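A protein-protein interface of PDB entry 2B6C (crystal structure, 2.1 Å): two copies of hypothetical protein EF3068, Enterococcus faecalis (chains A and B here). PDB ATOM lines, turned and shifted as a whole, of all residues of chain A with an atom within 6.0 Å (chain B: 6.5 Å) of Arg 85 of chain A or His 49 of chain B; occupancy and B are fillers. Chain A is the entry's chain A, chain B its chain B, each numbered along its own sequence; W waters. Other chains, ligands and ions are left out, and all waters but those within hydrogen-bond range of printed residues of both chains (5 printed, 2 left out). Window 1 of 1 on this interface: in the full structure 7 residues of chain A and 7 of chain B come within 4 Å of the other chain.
Printed residues of chain A that touch a printed residue of chain B: His 49, Thr 50, Gln 84, Arg 85 and Phe 86. Along chain A the printed residues that touch a printed residue of chain B span positions 49 to 86. Of the 15 printed residues of chain B, 3 touch a printed residue of chain A.
Arg 85 of chain A touches two residues of chain B. Of chain A, only Gln 84 and Arg 85 come within 4 Å of His 49 of chain B. Of the printed residues of chain B, Gln 84 of chain A touches His 49 and Thr 50. Printed residues of chain A within 4 Å of Arg 85 of chain B: His 49 and Thr 50. Printed residues of chain B within 4 Å of Thr 50 of chain A: Arg 85. Of the printed residues of chain B, Phe 86 of chain A touches Thr 50. Of the printed residues of chain A, Thr 50 of chain B touches Gln 84, Arg 85 and Phe 86. The nearest residue of chain B that does not touch Arg 85 of chain A is Arg 85 of chain B (4.04 Å). The nearest residue of chain A that does not touch His 49 of chain B is Phe 86 of chain A (5.3 Å). The nearest printed residue of chain B that does not touch Thr 50 of chain A is Lys 53 of chain B (4.03 Å).
O of Trp 51 of chain A sits at hydrogen-bond distance from NH2 of Arg 85 of chain A (2.7 Å). A ring nitrogen (NE2) of His 49 of chain B lies within hydrogen-bond range of the backbone carbonyl oxygen (O) of Gln 81 of chain B, at 3.1 Å. The guanidinium group (NH1) of Arg 85 of chain A sits close to the side-chain amide oxygen (OD1) of Asn 82 of chain A, at 3.5 Å. The backbone carbonyl oxygen (O) of Ser 48 of chain B lies within hydrogen-bond range of the guanidinium group (NH1) of Arg 85 of chain B. The backbone carbonyl oxygen (O) of Ser 48 of chain A sits at hydrogen-bond distance from the guanidinium group (NH1) of Arg 85 of chain A (3.0 Å). O of Glu 47 of chain B sits at hydrogen-bond distance from OG1 of Thr 50 of chain B (2.8 Å).
His 49 of chain A touches Arg 85 of chain B, and with the chains exchanged Arg 85 of chain A touches His 49 of chain B. Thr 50 of chain A touches Arg 85 of chain B, and with the chains exchanged Arg 85 of chain A touches Thr 50 of chain B. 9 positions are printed for both chains.
Among the printed residues, pairs that only touch across the chains: His 49 of chain A with Arg 85 of chain B (3.4 Å), Thr 50 of chain A with Arg 85 of chain B (3.3 Å), Gln 84 of chain A with His 49 of chain B (3.2 Å), Gln 84 of chain A with Thr 50 of chain B (3.5 Å), Arg 85 of chain A with His 49 of chain B (3.2 Å), Arg 85 of chain A with Thr 50 of chain B (3.3 Å) and Phe 86 of chain A with Thr 50 of chain B (3.9 Å).
Water W4 bridges O of Thr 50 of chain A (2.7 Å) and NZ of Lys 53 of chain B (3.1 Å). Water W1 bridges O of Thr 50 of chain B and NZ of Lys 53 of chain A. Water W5 lies within hydrogen-bond range of the backbone carbonyl oxygen of His 49 of chain B (2.8 Å) and the guanidinium group of Arg 85 of chain A (3.1 Å). Water W2 bridges O of Gln 84 of chain A (2.8 Å) and O of Lys 46 of chain B (2.9 Å). Water W3 bridges NH2 of Arg 85 of chain B (3.1 Å) and NH2 of Arg 85 of chain A (3.2 Å).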
ATOM      1  N   SER A  48      -4.428  29.039  31.565  1.00  0.00           N
ATOM      2  CA  SER A  48      -4.504  29.175  30.105  1.00  0.00           C
ATOM      3  C   SER A  48      -5.097  27.970  29.373  1.00  0.00           C
ATOM      4  O   SER A  48      -5.723  28.148  28.297  1.00  0.00           O
ATOM      5  CB  SER A  48      -3.136  29.564  29.499  1.00  0.00           C
ATOM      6  OG  SER A  48      -2.259  28.459  29.303  1.00  0.00           O
ATOM      7  N   HIS A  49      -4.908  26.756  29.932  1.00  0.00           N
ATOM      8  CA  HIS A  49      -5.466  25.538  29.299  1.00  0.00           C
ATOM      9  C   HIS A  49      -6.999  25.552  29.262  1.00  0.00           C
ATOM     10  O   HIS A  49      -7.599  24.925  28.405  1.00  0.00           O
ATOM     11  CB  HIS A  49      -4.972  24.262  29.988  1.00  0.00           C
ATOM     12  CG  HIS A  49      -3.483  24.062  29.894  1.00  0.00           C
ATOM     13  ND1 HIS A  49      -2.623  24.355  30.927  1.00  0.00           N
ATOM     14  CD2 HIS A  49      -2.711  23.573  28.898  1.00  0.00           C
ATOM     15  CE1 HIS A  49      -1.383  24.102  30.562  1.00  0.00           C
ATOM     16  NE2 HIS A  49      -1.408  23.608  29.338  1.00  0.00           N
ATOM     17  N   THR A  50      -7.606  26.283  30.195  1.00  0.00           N
ATOM     18  CA  THR A  50      -9.051  26.342  30.348  1.00  0.00           C
ATOM     19  C   THR A  50      -9.722  27.479  29.554  1.00  0.00           C
ATOM     20  O   THR A  50     -10.940  27.527  29.470  1.00  0.00           O
ATOM     21  CB  THR A  50      -9.435  26.554  31.796  1.00  0.00           C
ATOM     22  OG1 THR A  50      -9.276  27.950  32.105  1.00  0.00           O
ATOM     23  CG2 THR A  50      -8.609  25.676  32.724  1.00  0.00           C
ATOM     24  N   TRP A  51      -8.930  28.381  28.978  1.00  0.00           N
ATOM     25  CA  TRP A  51      -9.460  29.548  28.249  1.00  0.00           C
ATOM     26  C   TRP A  51      -9.998  29.180  26.887  1.00  0.00           C
ATOM     27  O   TRP A  51      -9.341  28.429  26.151  1.00  0.00           O
ATOM     28  CB  TRP A  51      -8.370  30.577  27.980  1.00  0.00           C
ATOM     29  CG  TRP A  51      -7.768  31.173  29.176  1.00  0.00           C
ATOM     30  CD1 TRP A  51      -8.286  31.206  30.447  1.00  0.00           C
ATOM     31  CD2 TRP A  51      -6.526  31.874  29.222  1.00  0.00           C
ATOM     32  NE1 TRP A  51      -7.417  31.871  31.286  1.00  0.00           N
ATOM     33  CE2 TRP A  51      -6.326  32.282  30.559  1.00  0.00           C
ATOM     34  CE3 TRP A  51      -5.535  32.159  28.268  1.00  0.00           C
ATOM     35  CZ2 TRP A  51      -5.195  33.001  30.959  1.00  0.00           C
ATOM     36  CZ3 TRP A  51      -4.415  32.870  28.670  1.00  0.00           C
ATOM     37  CH2 TRP A  51      -4.266  33.294  30.001  1.00  0.00           C
ATOM     38  N   PRO A  52     -11.121  29.794  26.494  1.00  0.00           N
ATOM     39  CA  PRO A  52     -11.533  29.672  25.101  1.00  0.00           C
ATOM     40  C   PRO A  52     -10.387  30.086  24.173  1.00  0.00           C
ATOM     41  O   PRO A  52      -9.572  30.953  24.532  1.00  0.00           O
ATOM     42  CB  PRO A  52     -12.684  30.665  24.997  1.00  0.00           C
ATOM     43  CG  PRO A  52     -13.263  30.749  26.414  1.00  0.00           C
ATOM     44  CD  PRO A  52     -12.029  30.678  27.267  1.00  0.00           C
ATOM     45  N   LYS A  53     -10.324  29.468  22.999  1.00  0.00           N
ATOM     46  CA  LYS A  53      -9.298  29.746  22.024  1.00  0.00           C
ATOM     47  C   LYS A  53      -9.083  31.274  21.756  1.00  0.00           C
ATOM     48  O   LYS A  53      -7.940  31.754  21.737  1.00  0.00           O
ATOM     49  CB  LYS A  53      -9.621  28.969  20.739  1.00  0.00           C
ATOM     50  CG  LYS A  53      -8.468  28.771  19.761  1.00  0.00           C
ATOM     51  CD  LYS A  53      -7.257  28.001  20.328  1.00  0.00           C
ATOM     52  CE  LYS A  53      -7.472  26.469  20.452  1.00  0.00           C
ATOM     53  NZ  LYS A  53      -7.842  25.719  19.183  1.00  0.00           N
ATOM     54  N   LEU A  56      -7.297  32.886  24.506  1.00  0.00           N
ATOM     55  CA  LEU A  56      -5.906  32.450  24.480  1.00  0.00           C
ATOM     56  C   LEU A  56      -5.091  33.237  23.437  1.00  0.00           C
ATOM     57  O   LEU A  56      -4.022  33.756  23.755  1.00  0.00           O
ATOM     58  CB  LEU A  56      -5.795  30.943  24.260  1.00  0.00           C
ATOM     59  CG  LEU A  56      -4.376  30.365  24.159  1.00  0.00           C
ATOM     60  CD1 LEU A  56      -3.592  30.534  25.490  1.00  0.00           C
ATOM     61  CD2 LEU A  56      -4.438  28.891  23.723  1.00  0.00           C
ATOM     62  N   ASN A  82      -0.018  25.118  25.312  1.00  0.00           N
ATOM     63  CA  ASN A  82      -1.290  24.799  24.669  1.00  0.00           C
ATOM     64  C   ASN A  82      -1.155  24.229  23.251  1.00  0.00           C
ATOM     65  O   ASN A  82      -2.087  24.302  22.456  1.00  0.00           O
ATOM     66  CB  ASN A  82      -2.156  26.062  24.649  1.00  0.00           C
ATOM     67  CG  ASN A  82      -2.675  26.403  26.015  1.00  0.00           C
ATOM     68  OD1 ASN A  82      -3.647  25.797  26.476  1.00  0.00           O
ATOM     69  ND2 ASN A  82      -2.022  27.346  26.698  1.00  0.00           N
ATOM     70  N   VAL A  83       0.013  23.669  22.935  1.00  0.00           N
ATOM     71  CA  VAL A  83       0.350  23.286  21.580  1.00  0.00           C
ATOM     72  C   VAL A  83      -0.604  22.199  21.029  1.00  0.00           C
ATOM     73  O   VAL A  83      -0.937  22.195  19.840  1.00  0.00           O
ATOM     74  CB  VAL A  83       1.846  22.848  21.471  1.00  0.00           C
ATOM     75  CG1 VAL A  83       2.120  21.554  22.298  1.00  0.00           C
ATOM     76  CG2 VAL A  83       2.228  22.677  20.025  1.00  0.00           C
ATOM     77  N   GLN A  84      -1.069  21.308  21.904  1.00  0.00           N
ATOM     78  CA  GLN A  84      -2.025  20.271  21.513  1.00  0.00           C
ATOM     79  C   GLN A  84      -3.419  20.800  21.106  1.00  0.00           C
ATOM     80  O   GLN A  84      -4.157  20.092  20.415  1.00  0.00           O
ATOM     81  CB  GLN A  84      -2.201  19.267  22.649  1.00  0.00           C
ATOM     82  CG  GLN A  84      -1.032  18.419  22.888  1.00  0.00           C
ATOM     83  CD  GLN A  84      -1.369  17.229  23.809  1.00  0.00           C
ATOM     84  OE1 GLN A  84      -1.653  17.407  25.007  1.00  0.00           O
ATOM     85  NE2 GLN A  84      -1.353  16.021  23.238  1.00  0.00           N
ATOM     86  N   ARG A  85      -3.746  22.035  21.515  1.00  0.00           N
ATOM     87  CA  ARG A  85      -5.075  22.639  21.320  1.00  0.00           C
ATOM     88  C   ARG A  85      -5.245  23.275  19.945  1.00  0.00           C
ATOM     89  O   ARG A  85      -6.371  23.522  19.510  1.00  0.00           O
ATOM     90  CB  ARG A  85      -5.346  23.708  22.396  1.00  0.00           C
ATOM     91  CG  ARG A  85      -5.522  23.151  23.828  1.00  0.00           C
ATOM     92  CD  ARG A  85      -5.862  24.267  24.857  1.00  0.00           C
ATOM     93  NE  ARG A  85      -7.116  24.891  24.517  1.00  0.00           N
ATOM     94  CZ  ARG A  85      -7.589  26.033  24.981  1.00  0.00           C
ATOM     95  NH1 ARG A  85      -6.914  26.814  25.831  1.00  0.00           N
ATOM     96  NH2 ARG A  85      -8.776  26.394  24.545  1.00  0.00           N
ATOM     97  N   PHE A  86      -4.132  23.511  19.248  1.00  0.00           N
ATOM     98  CA  PHE A  86      -4.162  24.238  17.962  1.00  0.00           C
ATOM     99  C   PHE A  86      -4.382  23.387  16.745  1.00  0.00           C
ATOM    100  O   PHE A  86      -3.749  22.351  16.586  1.00  0.00           O
ATOM    101  CB  PHE A  86      -2.900  25.099  17.764  1.00  0.00           C
ATOM    102  CG  PHE A  86      -2.719  26.134  18.841  1.00  0.00           C
ATOM    103  CD1 PHE A  86      -3.664  27.149  19.007  1.00  0.00           C
ATOM    104  CD2 PHE A  86      -1.661  26.051  19.725  1.00  0.00           C
ATOM    105  CE1 PHE A  86      -3.525  28.095  20.014  1.00  0.00           C
ATOM    106  CE2 PHE A  86      -1.490  26.995  20.726  1.00  0.00           C
ATOM    107  CZ  PHE A  86      -2.426  28.024  20.871  1.00  0.00           C
ATOM    108  N   SER A  87      -5.285  23.848  15.890  1.00  0.00           N
ATOM    109  CA  SER A  87      -5.438  23.317  14.538  1.00  0.00           C
ATOM    110  C   SER A  87      -4.305  23.759  13.622  1.00  0.00           C
ATOM    111  O   SER A  87      -3.539  24.668  13.944  1.00  0.00           O
ATOM    112  CB  SER A  87      -6.741  23.832  13.929  1.00  0.00           C
ATOM    113  OG  SER A  87      -6.684  25.240  13.812  1.00  0.00           O
ATOM    114  N   GLU A  90      -4.636  27.558  12.915  1.00  0.00           N
ATOM    115  CA  GLU A  90      -4.151  28.392  14.012  1.00  0.00           C
ATOM    116  C   GLU A  90      -2.625  28.393  14.080  1.00  0.00           C
ATOM    117  O   GLU A  90      -2.007  29.429  14.319  1.00  0.00           O
ATOM    118  CB  GLU A  90      -4.768  27.948  15.354  1.00  0.00           C
ATOM    119  CG  GLU A  90      -6.250  28.301  15.483  1.00  0.00           C
ATOM    120  CD  GLU A  90      -7.038  27.436  16.491  1.00  0.00           C
ATOM    121  OE1 GLU A  90      -6.571  26.371  16.945  1.00  0.00           O
ATOM    122  OE2 GLU A  90      -8.186  27.826  16.789  1.00  0.00           O
ATOM    123  N   LEU B  44      -8.719  10.000  17.623  1.00  0.00           N
ATOM    124  CA  LEU B  44      -9.816  10.773  18.170  1.00  0.00           C
ATOM    125  C   LEU B  44      -9.364  11.533  19.418  1.00  0.00           C
ATOM    126  O   LEU B  44      -9.739  12.698  19.610  1.00  0.00           O
ATOM    127  CB  LEU B  44     -11.039   9.865  18.483  1.00  0.00           C
ATOM    128  CG  LEU B  44     -12.170  10.515  19.280  1.00  0.00           C
ATOM    129  CD1 LEU B  44     -13.073  11.282  18.345  1.00  0.00           C
ATOM    130  CD2 LEU B  44     -12.917   9.413  19.974  1.00  0.00           C
ATOM    131  N   LEU B  45      -8.572  10.880  20.275  1.00  0.00           N
ATOM    132  CA  LEU B  45      -8.110  11.529  21.490  1.00  0.00           C
ATOM    133  C   LEU B  45      -7.203  12.716  21.130  1.00  0.00           C
ATOM    134  O   LEU B  45      -7.268  13.757  21.771  1.00  0.00           O
ATOM    135  CB  LEU B  45      -7.422  10.534  22.444  1.00  0.00           C
ATOM    136  CG  LEU B  45      -8.371   9.444  22.992  1.00  0.00           C
ATOM    137  CD1 LEU B  45      -7.599   8.439  23.848  1.00  0.00           C
ATOM    138  CD2 LEU B  45      -9.522  10.010  23.802  1.00  0.00           C
ATOM    139  N   LYS B  46      -6.365  12.540  20.112  1.00  0.00           N
ATOM    140  CA  LYS B  46      -5.481  13.606  19.648  1.00  0.00           C
ATOM    141  C   LYS B  46      -6.268  14.834  19.173  1.00  0.00           C
ATOM    142  O   LYS B  46      -5.953  15.953  19.543  1.00  0.00           O
ATOM    143  CB  LYS B  46      -4.550  13.086  18.546  1.00  0.00           C
ATOM    144  CG  LYS B  46      -3.787  14.163  17.765  1.00  0.00           C
ATOM    145  CD  LYS B  46      -2.994  13.569  16.585  1.00  0.00           C
ATOM    146  CE  LYS B  46      -1.845  12.693  17.040  1.00  0.00           C
ATOM    147  NZ  LYS B  46      -0.838  12.459  15.954  1.00  0.00           N
ATOM    148  N   GLU B  47      -7.293  14.636  18.344  1.00  0.00           N
ATOM    149  CA  GLU B  47      -8.018  15.788  17.805  1.00  0.00           C
ATOM    150  C   GLU B  47      -8.931  16.444  18.845  1.00  0.00           C
ATOM    151  O   GLU B  47      -9.275  17.604  18.704  1.00  0.00           O
ATOM    152  CB  GLU B  47      -8.747  15.460  16.479  1.00  0.00           C
ATOM    153  CG  GLU B  47     -10.261  15.261  16.550  1.00  0.00           C
ATOM    154  CD  GLU B  47     -10.962  15.475  15.208  1.00  0.00           C
ATOM    155  OE1 GLU B  47     -10.267  15.465  14.166  1.00  0.00           O
ATOM    156  OE2 GLU B  47     -12.208  15.651  15.194  1.00  0.00           O
ATOM    157  N   SER B  48      -9.284  15.700  19.894  1.00  0.00           N
ATOM    158  CA  SER B  48     -10.174  16.201  20.936  1.00  0.00           C
ATOM    159  C   SER B  48      -9.608  17.445  21.645  1.00  0.00           C
ATOM    160  O   SER B  48     -10.363  18.310  22.046  1.00  0.00           O
ATOM    161  CB  SER B  48     -10.487  15.110  21.948  1.00  0.00           C
ATOM    162  OG  SER B  48      -9.374  14.914  22.821  1.00  0.00           O
ATOM    163  N   HIS B  49      -8.284  17.522  21.796  1.00  0.00           N
ATOM    164  CA  HIS B  49      -7.608  18.732  22.350  1.00  0.00           C
ATOM    165  C   HIS B  49      -7.902  20.007  21.582  1.00  0.00           C
ATOM    166  O   HIS B  49      -7.799  21.114  22.144  1.00  0.00           O
ATOM    167  CB  HIS B  49      -6.094  18.541  22.377  1.00  0.00           C
ATOM    168  CG  HIS B  49      -5.663  17.336  23.148  1.00  0.00           C
ATOM    169  ND1 HIS B  49      -5.164  16.204  22.541  1.00  0.00           N
ATOM    170  CD2 HIS B  49      -5.667  17.080  24.473  1.00  0.00           C
ATOM    171  CE1 HIS B  49      -4.889  15.298  23.456  1.00  0.00           C
ATOM    172  NE2 HIS B  49      -5.190  15.802  24.637  1.00  0.00           N
ATOM    173  N   THR B  50      -8.272  19.853  20.308  1.00  0.00           N
ATOM    174  CA  THR B  50      -8.499  21.006  19.427  1.00  0.00           C
ATOM    175  C   THR B  50      -9.969  21.473  19.425  1.00  0.00           C
ATOM    176  O   THR B  50     -10.289  22.542  18.905  1.00  0.00           O
ATOM    177  CB  THR B  50      -8.000  20.739  17.938  1.00  0.00           C
ATOM    178  OG1 THR B  50      -8.947  19.937  17.230  1.00  0.00           O
ATOM    179  CG2 THR B  50      -6.629  20.053  17.897  1.00  0.00           C
ATOM    180  N   TRP B  51     -10.861  20.659  19.974  1.00  0.00           N
ATOM    181  CA  TRP B  51     -12.286  20.967  19.960  1.00  0.00           C
ATOM    182  C   TRP B  51     -12.607  22.122  20.893  1.00  0.00           C
ATOM    183  O   TRP B  51     -12.025  22.217  21.977  1.00  0.00           O
ATOM    184  CB  TRP B  51     -13.167  19.765  20.352  1.00  0.00           C
ATOM    185  CG  TRP B  51     -13.032  18.543  19.477  1.00  0.00           C
ATOM    186  CD1 TRP B  51     -12.588  18.479  18.158  1.00  0.00           C
ATOM    187  CD2 TRP B  51     -13.392  17.210  19.837  1.00  0.00           C
ATOM    188  NE1 TRP B  51     -12.611  17.164  17.718  1.00  0.00           N
ATOM    189  CE2 TRP B  51     -13.110  16.373  18.717  1.00  0.00           C
ATOM    190  CE3 TRP B  51     -13.882  16.628  21.012  1.00  0.00           C
ATOM    191  CZ2 TRP B  51     -13.312  14.991  18.752  1.00  0.00           C
ATOM    192  CZ3 TRP B  51     -14.090  15.270  21.035  1.00  0.00           C
ATOM    193  CH2 TRP B  51     -13.790  14.461  19.921  1.00  0.00           C
ATOM    194  N   PRO B  52     -13.559  22.989  20.475  1.00  0.00           N
ATOM    195  CA  PRO B  52     -14.110  23.973  21.401  1.00  0.00           C
ATOM    196  C   PRO B  52     -14.634  23.229  22.621  1.00  0.00           C
ATOM    197  O   PRO B  52     -15.025  22.044  22.522  1.00  0.00           O
ATOM    198  CB  PRO B  52     -15.233  24.626  20.603  1.00  0.00           C
ATOM    199  CG  PRO B  52     -14.796  24.414  19.109  1.00  0.00           C
ATOM    200  CD  PRO B  52     -14.169  23.061  19.126  1.00  0.00           C
ATOM    201  N   LYS B  53     -14.572  23.883  23.774  1.00  0.00           N
ATOM    202  CA  LYS B  53     -15.022  23.285  25.026  1.00  0.00           C
ATOM    203  C   LYS B  53     -16.422  22.672  24.901  1.00  0.00           C
ATOM    204  O   LYS B  53     -16.665  21.564  25.384  1.00  0.00           O
ATOM    205  CB  LYS B  53     -14.992  24.325  26.160  1.00  0.00           C
ATOM    206  CG  LYS B  53     -15.361  23.768  27.574  1.00  0.00           C
ATOM    207  CD  LYS B  53     -14.480  22.564  28.022  1.00  0.00           C
ATOM    208  CE  LYS B  53     -12.989  22.902  28.175  1.00  0.00           C
ATOM    209  NZ  LYS B  53     -12.766  23.947  29.234  1.00  0.00           N
ATOM    210  N   LEU B  56     -16.329  19.424  23.103  1.00  0.00           N
ATOM    211  CA  LEU B  56     -15.700  18.411  23.948  1.00  0.00           C
ATOM    212  C   LEU B  56     -16.692  17.816  24.958  1.00  0.00           C
ATOM    213  O   LEU B  56     -16.775  16.596  25.095  1.00  0.00           O
ATOM    214  CB  LEU B  56     -14.438  18.946  24.655  1.00  0.00           C
ATOM    215  CG  LEU B  56     -13.685  17.996  25.626  1.00  0.00           C
ATOM    216  CD1 LEU B  56     -13.272  16.641  24.984  1.00  0.00           C
ATOM    217  CD2 LEU B  56     -12.496  18.706  26.259  1.00  0.00           C
ATOM    218  N   LEU B  78     -11.510  10.726  26.926  1.00  0.00           N
ATOM    219  CA  LEU B  78     -11.621  12.098  26.419  1.00  0.00           C
ATOM    220  C   LEU B  78     -11.445  13.141  27.530  1.00  0.00           C
ATOM    221  O   LEU B  78     -10.767  14.170  27.346  1.00  0.00           O
ATOM    222  CB  LEU B  78     -12.955  12.340  25.694  1.00  0.00           C
ATOM    223  CG  LEU B  78     -13.056  11.678  24.321  1.00  0.00           C
ATOM    224  CD1 LEU B  78     -14.510  11.671  23.847  1.00  0.00           C
ATOM    225  CD2 LEU B  78     -12.196  12.426  23.304  1.00  0.00           C
ATOM    226  N   GLN B  81      -7.681  12.829  28.918  1.00  0.00           N
ATOM    227  CA  GLN B  81      -6.743  13.475  27.984  1.00  0.00           C
ATOM    228  C   GLN B  81      -6.796  15.003  27.987  1.00  0.00           C
ATOM    229  O   GLN B  81      -5.818  15.653  27.650  1.00  0.00           O
ATOM    230  CB  GLN B  81      -6.982  12.969  26.548  1.00  0.00           C
ATOM    231  CG  GLN B  81      -6.555  11.518  26.299  1.00  0.00           C
ATOM    232  CD  GLN B  81      -5.268  11.088  27.016  1.00  0.00           C
ATOM    233  OE1 GLN B  81      -5.309  10.470  28.095  1.00  0.00           O
ATOM    234  NE2 GLN B  81      -4.128  11.392  26.415  1.00  0.00           N
ATOM    235  N   ASN B  82      -7.951  15.563  28.321  1.00  0.00           N
ATOM    236  CA  ASN B  82      -8.163  16.997  28.308  1.00  0.00           C
ATOM    237  C   ASN B  82      -8.273  17.569  29.724  1.00  0.00           C
ATOM    238  O   ASN B  82      -8.815  18.657  29.921  1.00  0.00           O
ATOM    239  CB  ASN B  82      -9.419  17.330  27.486  1.00  0.00           C
ATOM    240  CG  ASN B  82      -9.232  17.017  26.008  1.00  0.00           C
ATOM    241  OD1 ASN B  82      -8.726  17.850  25.252  1.00  0.00           O
ATOM    242  ND2 ASN B  82      -9.627  15.807  25.590  1.00  0.00           N
ATOM    243  N   ARG B  85      -7.747  21.228  30.597  1.00  0.00           N
ATOM    244  CA  ARG B  85      -8.706  22.157  30.004  1.00  0.00           C
ATOM    245  C   ARG B  85      -9.917  22.492  30.887  1.00  0.00           C
ATOM    246  O   ARG B  85     -10.629  23.470  30.621  1.00  0.00           O
ATOM    247  CB  ARG B  85      -9.201  21.619  28.648  1.00  0.00           C
ATOM    248  CG  ARG B  85      -8.086  21.472  27.588  1.00  0.00           C
ATOM    249  CD  ARG B  85      -8.691  21.027  26.242  1.00  0.00           C
ATOM    250  NE  ARG B  85      -9.658  22.016  25.782  1.00  0.00           N
ATOM    251  CZ  ARG B  85     -10.514  21.872  24.779  1.00  0.00           C
ATOM    252  NH1 ARG B  85     -10.558  20.754  24.058  1.00  0.00           N
ATOM    253  NH2 ARG B  85     -11.339  22.867  24.496  1.00  0.00           N
HETATM  254  O   HOH W   1     -10.744  25.109  19.703  1.00  0.00           O
HETATM  255  O   HOH W   2      -3.542  17.622  19.291  1.00  0.00           O
HETATM  256  O   HOH W   3     -11.788  25.806  25.454  1.00  0.00           O
HETATM  257  O   HOH W   4     -12.785  26.680  27.720  1.00  0.00           O
HETATM  258  O   HOH W   5      -8.753  23.714  22.224  1.00  0.00           O
